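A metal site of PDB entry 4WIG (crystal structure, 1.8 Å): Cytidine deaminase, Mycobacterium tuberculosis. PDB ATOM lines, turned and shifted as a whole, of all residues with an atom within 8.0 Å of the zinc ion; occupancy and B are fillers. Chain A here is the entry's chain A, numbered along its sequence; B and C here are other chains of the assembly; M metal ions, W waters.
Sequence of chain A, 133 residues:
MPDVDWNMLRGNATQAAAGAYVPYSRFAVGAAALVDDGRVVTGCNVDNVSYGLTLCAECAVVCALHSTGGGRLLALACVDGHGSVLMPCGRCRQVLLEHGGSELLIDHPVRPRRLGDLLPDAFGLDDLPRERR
The side-chain sulfur (SG) of Cys 89 sits close to the backbone NH (N) of Arg 91 (3.7 Å). NH1 of Arg 91 lies close to SG of Cys 56 (3.3 Å). OE2 of Glu 58 sits close to SG of Cys 92 (3.8 Å). The guanidinium group of Arg 91 is in hydrogen-bond range of the backbone carbonyl oxygen of Thr 54. The side-chain hydroxyl (OG) of Ser 50 of chain B sits close to the side-chain sulfur (SG) of Cys 89 (3.4 Å).
Glu 58 touches the zinc ion. Arg 91 touches the zinc ion (NE to ZN, 3.9 Å). Of the 24 residues printed, 5 come within 4 Å of the zinc ion. The nearest printed residue that does not touch the zinc ion is Ser 50 of chain B (4.1 Å).
The zinc ion is bound by water W1 (1.9 Å), the side-chain sulfur of Cys 92 (2.3 Å), the side-chain sulfur of Cys 89 (2.3 Å) and the side-chain sulfur of Cys 56 (2.3 Å). The zinc ion has four donor atoms within binding distance.
Water W1 bridges the side-chain carboxylate (OE2) of Glu 58 (2.6 Å) and the backbone NH (N) of Cys 89 (3.0 Å).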
ATOM      1  N   VAL A  29     -12.277   5.120  -4.528  1.00  0.00           N
ATOM      2  CA  VAL A  29     -12.553   3.693  -4.399  1.00  0.00           C
ATOM      3  C   VAL A  29     -11.261   3.003  -4.046  1.00  0.00           C
ATOM      4  O   VAL A  29     -10.231   3.333  -4.583  1.00  0.00           O
ATOM      5  CB  VAL A  29     -13.127   3.096  -5.682  1.00  0.00           C
ATOM      6  CG1 VAL A  29     -13.347   1.599  -5.521  1.00  0.00           C
ATOM      7  CG2 VAL A  29     -14.435   3.797  -6.045  1.00  0.00           C
ATOM      8  N   ASN A  45      -8.704   3.680  -7.294  1.00  0.00           N
ATOM      9  CA  ASN A  45      -9.004   4.281  -8.596  1.00  0.00           C
ATOM     10  C   ASN A  45      -8.159   5.532  -8.928  1.00  0.00           C
ATOM     11  O   ASN A  45      -7.594   6.208  -8.054  1.00  0.00           O
ATOM     12  CB  ASN A  45     -10.518   4.505  -8.802  1.00  0.00           C
ATOM     13  CG  ASN A  45     -11.142   5.445  -7.787  1.00  0.00           C
ATOM     14  OD1 ASN A  45     -10.639   5.627  -6.693  1.00  0.00           O
ATOM     15  ND2 ASN A  45     -12.256   6.054  -8.172  1.00  0.00           N
ATOM     16  N   THR A  54      -9.937   6.413 -17.085  1.00  0.00           N
ATOM     17  CA  THR A  54      -9.937   6.182 -15.654  1.00  0.00           C
ATOM     18  C   THR A  54      -9.644   4.726 -15.355  1.00  0.00           C
ATOM     19  O   THR A  54     -10.160   3.827 -16.029  1.00  0.00           O
ATOM     20  CB  THR A  54     -11.289   6.589 -15.048  1.00  0.00           C
ATOM     21  OG1 THR A  54     -11.455   8.018 -15.182  1.00  0.00           O
ATOM     22  CG2 THR A  54     -11.383   6.208 -13.585  1.00  0.00           C
ATOM     23  N   LEU A  55      -8.780   4.496 -14.356  1.00  0.00           N
ATOM     24  CA  LEU A  55      -8.411   3.160 -13.897  1.00  0.00           C
ATOM     25  C   LEU A  55      -9.218   2.815 -12.654  1.00  0.00           C
ATOM     26  O   LEU A  55      -9.273   3.613 -11.717  1.00  0.00           O
ATOM     27  CB  LEU A  55      -6.903   3.127 -13.606  1.00  0.00           C
ATOM     28  CG  LEU A  55      -6.027   3.450 -14.818  1.00  0.00           C
ATOM     29  CD1 LEU A  55      -4.622   3.890 -14.433  1.00  0.00           C
ATOM     30  CD2 LEU A  55      -5.977   2.249 -15.746  1.00  0.00           C
ATOM     31  N   CYS A  56      -9.870   1.652 -12.658  1.00  0.00           N
ATOM     32  CA  CYS A  56     -10.616   1.164 -11.509  1.00  0.00           C
ATOM     33  C   CYS A  56      -9.702   0.562 -10.461  1.00  0.00           C
ATOM     34  O   CYS A  56      -8.678  -0.041 -10.800  1.00  0.00           O
ATOM     35  CB  CYS A  56     -11.622   0.101 -11.935  1.00  0.00           C
ATOM     36  SG  CYS A  56     -13.125   0.735 -12.716  1.00  0.00           S
ATOM     37  N   ALA A  57     -10.107   0.683  -9.198  1.00  0.00           N
ATOM     38  CA  ALA A  57      -9.369   0.086  -8.083  1.00  0.00           C
ATOM     39  C   ALA A  57      -9.090  -1.406  -8.279  1.00  0.00           C
ATOM     40  O   ALA A  57      -8.007  -1.890  -7.972  1.00  0.00           O
ATOM     41  CB  ALA A  57     -10.144   0.292  -6.775  1.00  0.00           C
ATOM     42  N   GLU A  58     -10.098  -2.128  -8.747  1.00  0.00           N
ATOM     43  CA  GLU A  58     -10.012  -3.559  -8.915  1.00  0.00           C
ATOM     44  C   GLU A  58      -8.990  -3.911  -9.998  1.00  0.00           C
ATOM     45  O   GLU A  58      -8.251  -4.898  -9.846  1.00  0.00           O
ATOM     46  CB  GLU A  58     -11.382  -4.168  -9.234  1.00  0.00           C
ATOM     47  CG  GLU A  58     -12.470  -3.784  -8.234  1.00  0.00           C
ATOM     48  CD  GLU A  58     -13.247  -2.549  -8.655  1.00  0.00           C
ATOM     49  OE1 GLU A  58     -12.647  -1.447  -8.780  1.00  0.00           O
ATOM     50  OE2 GLU A  58     -14.477  -2.651  -8.849  1.00  0.00           O
ATOM     51  N   CYS A  59      -8.926  -3.126 -11.062  1.00  0.00           N
ATOM     52  CA  CYS A  59      -7.875  -3.280 -12.062  1.00  0.00           C
ATOM     53  C   CYS A  59      -6.502  -2.984 -11.485  1.00  0.00           C
ATOM     54  O   CYS A  59      -5.539  -3.671 -11.806  1.00  0.00           O
ATOM     55  CB  CYS A  59      -8.119  -2.399 -13.284  1.00  0.00           C
ATOM     56  SG  CYS A  59      -9.529  -2.979 -14.259  1.00  0.00           S
ATOM     57  N   CYS A  78     -14.132  -4.379  -2.138  1.00  0.00           N
ATOM     58  CA  CYS A  78     -14.085  -3.063  -2.784  1.00  0.00           C
ATOM     59  C   CYS A  78     -14.979  -2.110  -1.992  1.00  0.00           C
ATOM     60  O   CYS A  78     -16.118  -2.441  -1.706  1.00  0.00           O
ATOM     61  CB  CYS A  78     -14.613  -3.162  -4.207  1.00  0.00           C
ATOM     62  SG  CYS A  78     -14.472  -1.647  -5.178  1.00  0.00           S
ATOM     63  N   MET A  87     -20.086  -3.096  -5.305  1.00  0.00           N
ATOM     64  CA  MET A  87     -19.996  -4.179  -6.280  1.00  0.00           C
ATOM     65  C   MET A  87     -19.136  -3.676  -7.440  1.00  0.00           C
ATOM     66  O   MET A  87     -19.296  -2.531  -7.876  1.00  0.00           O
ATOM     67  CB  MET A  87     -21.370  -4.572  -6.811  1.00  0.00           C
ATOM     68  CG  MET A  87     -22.282  -5.311  -5.855  1.00  0.00           C
ATOM     69  SD  MET A  87     -21.586  -6.860  -5.263  1.00  0.00           S
ATOM     70  CE  MET A  87     -20.938  -6.244  -3.710  1.00  0.00           C
ATOM     71  N   PRO A  88     -18.215  -4.516  -7.942  1.00  0.00           N
ATOM     72  CA  PRO A  88     -17.398  -4.064  -9.078  1.00  0.00           C
ATOM     73  C   PRO A  88     -18.200  -3.793 -10.329  1.00  0.00           C
ATOM     74  O   PRO A  88     -19.252  -4.416 -10.544  1.00  0.00           O
ATOM     75  CB  PRO A  88     -16.450  -5.243  -9.322  1.00  0.00           C
ATOM     76  CG  PRO A  88     -16.317  -5.873  -7.993  1.00  0.00           C
ATOM     77  CD  PRO A  88     -17.620  -5.697  -7.294  1.00  0.00           C
ATOM     78  N   CYS A  89     -17.717  -2.883 -11.158  1.00  0.00           N
ATOM     79  CA  CYS A  89     -18.354  -2.605 -12.425  1.00  0.00           C
ATOM     80  C   CYS A  89     -18.101  -3.801 -13.334  1.00  0.00           C
ATOM     81  O   CYS A  89     -17.250  -4.623 -13.041  1.00  0.00           O
ATOM     82  CB  CYS A  89     -17.824  -1.320 -13.068  1.00  0.00           C
ATOM     83  SG  CYS A  89     -16.232  -1.387 -13.915  1.00  0.00           S
ATOM     84  N   GLY A  90     -18.866  -3.872 -14.413  1.00  0.00           N
ATOM     85  CA  GLY A  90     -18.824  -5.031 -15.312  1.00  0.00           C
ATOM     86  C   GLY A  90     -17.438  -5.303 -15.878  1.00  0.00           C
ATOM     87  O   GLY A  90     -17.053  -6.458 -16.021  1.00  0.00           O
ATOM     88  N   ARG A  91     -16.718  -4.232 -16.198  1.00  0.00           N
ATOM     89  CA  ARG A  91     -15.357  -4.321 -16.743  1.00  0.00           C
ATOM     90  C   ARG A  91     -14.480  -5.043 -15.742  1.00  0.00           C
ATOM     91  O   ARG A  91     -13.789  -6.012 -16.058  1.00  0.00           O
ATOM     92  CB  ARG A  91     -14.832  -2.899 -17.038  1.00  0.00           C
ATOM     93  CG  ARG A  91     -13.383  -2.793 -17.508  1.00  0.00           C
ATOM     94  CD  ARG A  91     -12.420  -2.495 -16.372  1.00  0.00           C
ATOM     95  NE  ARG A  91     -12.552  -1.138 -15.829  1.00  0.00           N
ATOM     96  CZ  ARG A  91     -12.025  -0.038 -16.392  1.00  0.00           C
ATOM     97  NH1 ARG A  91     -12.190   1.142 -15.806  1.00  0.00           N
ATOM     98  NH2 ARG A  91     -11.362  -0.119 -17.542  1.00  0.00           N
ATOM     99  N   CYS A  92     -14.525  -4.569 -14.503  1.00  0.00           N
ATOM    100  CA  CYS A  92     -13.778  -5.172 -13.410  1.00  0.00           C
ATOM    101  C   CYS A  92     -14.199  -6.606 -13.110  1.00  0.00           C
ATOM    102  O   CYS A  92     -13.346  -7.438 -12.782  1.00  0.00           O
ATOM    103  CB  CYS A  92     -13.892  -4.290 -12.170  1.00  0.00           C
ATOM    104  SG  CYS A  92     -12.961  -2.771 -12.319  1.00  0.00           S
ATOM    105  N   ARG A  93     -15.486  -6.932 -13.252  1.00  0.00           N
ATOM    106  CA  ARG A  93     -15.902  -8.328 -13.107  1.00  0.00           C
ATOM    107  C   ARG A  93     -15.193  -9.210 -14.139  1.00  0.00           C
ATOM    108  O   ARG A  93     -14.706 -10.286 -13.799  1.00  0.00           O
ATOM    109  CB  ARG A  93     -17.421  -8.456 -13.200  1.00  0.00           C
ATOM    110  CG  ARG A  93     -18.125  -7.867 -11.998  1.00  0.00           C
ATOM    111  CD  ARG A  93     -19.648  -8.013 -12.027  1.00  0.00           C
ATOM    112  NE  ARG A  93     -20.265  -7.046 -11.130  1.00  0.00           N
ATOM    113  CZ  ARG A  93     -21.537  -7.034 -10.754  1.00  0.00           C
ATOM    114  NH1 ARG A  93     -22.387  -7.946 -11.183  1.00  0.00           N
ATOM    115  NH2 ARG A  93     -21.959  -6.088  -9.942  1.00  0.00           N
ATOM    116  N   VAL A  95     -12.265  -8.498 -15.756  1.00  0.00           N
ATOM    117  CA  VAL A  95     -10.844  -8.503 -15.440  1.00  0.00           C
ATOM    118  C   VAL A  95     -10.537  -9.443 -14.256  1.00  0.00           C
ATOM    119  O   VAL A  95      -9.628 -10.259 -14.324  1.00  0.00           O
ATOM    120  CB  VAL A  95     -10.299  -7.071 -15.174  1.00  0.00           C
ATOM    121  CG1 VAL A  95      -8.862  -7.113 -14.669  1.00  0.00           C
ATOM    122  CG2 VAL A  95     -10.367  -6.234 -16.446  1.00  0.00           C
ATOM    123  N   LEU A  96     -11.327  -9.342 -13.181  1.00  0.00           N
ATOM    124  CA  LEU A  96     -11.096 -10.182 -11.991  1.00  0.00           C
ATOM    125  C   LEU A  96     -11.286 -11.675 -12.312  1.00  0.00           C
ATOM    126  O   LEU A  96     -10.578 -12.531 -11.766  1.00  0.00           O
ATOM    127  CB  LEU A  96     -12.009  -9.745 -10.848  1.00  0.00           C
ATOM    128  CG  LEU A  96     -11.691  -8.408 -10.166  1.00  0.00           C
ATOM    129  CD1 LEU A  96     -12.817  -7.984  -9.217  1.00  0.00           C
ATOM    130  CD2 LEU A  96     -10.370  -8.508  -9.448  1.00  0.00           C
ATOM    131  N   SER B  50     -19.702   3.978 -14.625  1.00  0.00           N
ATOM    132  CA  SER B  50     -18.276   3.702 -14.372  1.00  0.00           C
ATOM    133  C   SER B  50     -17.534   4.543 -15.402  1.00  0.00           C
ATOM    134  O   SER B  50     -17.491   4.194 -16.575  1.00  0.00           O
ATOM    135  CB  SER B  50     -17.940   2.211 -14.522  1.00  0.00           C
ATOM    136  OG  SER B  50     -16.582   1.943 -14.198  1.00  0.00           O
ATOM    137  N   TYR B  51     -16.980   5.674 -14.972  1.00  0.00           N
ATOM    138  CA  TYR B  51     -16.440   6.668 -15.922  1.00  0.00           C
ATOM    139  C   TYR B  51     -15.392   6.109 -16.887  1.00  0.00           C
ATOM    140  O   TYR B  51     -15.311   6.566 -18.036  1.00  0.00           O
ATOM    141  CB  TYR B  51     -15.848   7.866 -15.180  1.00  0.00           C
ATOM    142  CG  TYR B  51     -16.843   8.786 -14.482  1.00  0.00           C
ATOM    143  CD1 TYR B  51     -18.179   8.425 -14.290  1.00  0.00           C
ATOM    144  CD2 TYR B  51     -16.426  10.017 -13.996  1.00  0.00           C
ATOM    145  CE1 TYR B  51     -19.073   9.272 -13.637  1.00  0.00           C
ATOM    146  CE2 TYR B  51     -17.307  10.877 -13.351  1.00  0.00           C
ATOM    147  CZ  TYR B  51     -18.615  10.512 -13.170  1.00  0.00           C
ATOM    148  OH  TYR B  51     -19.481  11.383 -12.510  1.00  0.00           O
ATOM    149  N   GLY B  52     -14.600   5.144 -16.446  1.00  0.00           N
ATOM    150  CA  GLY B  52     -13.577   4.516 -17.288  1.00  0.00           C
ATOM    151  C   GLY B  52     -14.087   3.699 -18.461  1.00  0.00           C
ATOM    152  O   GLY B  52     -13.304   3.147 -19.234  1.00  0.00           O
ATOM    153  N   LEU B  53     -15.411   3.588 -18.579  1.00  0.00           N
ATOM    154  CA  LEU B  53     -16.037   2.898 -19.722  1.00  0.00           C
ATOM    155  C   LEU B  53     -16.657   3.887 -20.679  1.00  0.00           C
ATOM    156  O   LEU B  53     -17.343   3.498 -21.629  1.00  0.00           O
ATOM    157  CB  LEU B  53     -17.073   1.887 -19.234  1.00  0.00           C
ATOM    158  CG  LEU B  53     -16.642   0.991 -18.075  1.00  0.00           C
ATOM    159  CD1 LEU B  53     -17.694  -0.106 -17.868  1.00  0.00           C
ATOM    160  CD2 LEU B  53     -15.256   0.398 -18.251  1.00  0.00           C
ATOM    161  N   GLN C  94     -21.884  -3.709 -18.641  1.00  0.00           N
ATOM    162  CA  GLN C  94     -22.035  -2.456 -17.895  1.00  0.00           C
ATOM    163  C   GLN C  94     -22.472  -1.342 -18.831  1.00  0.00           C
ATOM    164  O   GLN C  94     -23.397  -0.588 -18.540  1.00  0.00           O
ATOM    165  CB  GLN C  94     -20.734  -2.081 -17.216  1.00  0.00           C
ATOM    166  CG  GLN C  94     -20.824  -0.880 -16.282  1.00  0.00           C
ATOM    167  CD  GLN C  94     -21.497  -1.205 -14.961  1.00  0.00           C
ATOM    168  OE1 GLN C  94     -21.140  -2.206 -14.302  1.00  0.00           O
ATOM    169  NE2 GLN C  94     -22.440  -0.375 -14.561  1.00  0.00           N
ATOM    170  N   PHE C 123     -23.070  -2.265 -10.361  1.00  0.00           N
ATOM    171  CA  PHE C 123     -22.580  -0.939  -9.980  1.00  0.00           C
ATOM    172  C   PHE C 123     -23.438   0.121 -10.701  1.00  0.00           C
ATOM    173  O   PHE C 123     -23.795  -0.069 -11.864  1.00  0.00           O
ATOM    174  CB  PHE C 123     -21.094  -0.774 -10.350  1.00  0.00           C
ATOM    175  CG  PHE C 123     -20.546   0.607 -10.084  1.00  0.00           C
ATOM    176  CD1 PHE C 123     -20.078   0.952  -8.846  1.00  0.00           C
ATOM    177  CD2 PHE C 123     -20.563   1.568 -11.082  1.00  0.00           C
ATOM    178  CE1 PHE C 123     -19.618   2.241  -8.593  1.00  0.00           C
ATOM    179  CE2 PHE C 123     -20.072   2.840 -10.857  1.00  0.00           C
ATOM    180  CZ  PHE C 123     -19.611   3.179  -9.616  1.00  0.00           C
HETATM  181 ZN    ZN M   1     -14.500  -1.101 -12.429  1.00  0.00          ZN
HETATM  182  O   HOH W   1     -15.348  -1.083 -10.695  1.00  0.00           O
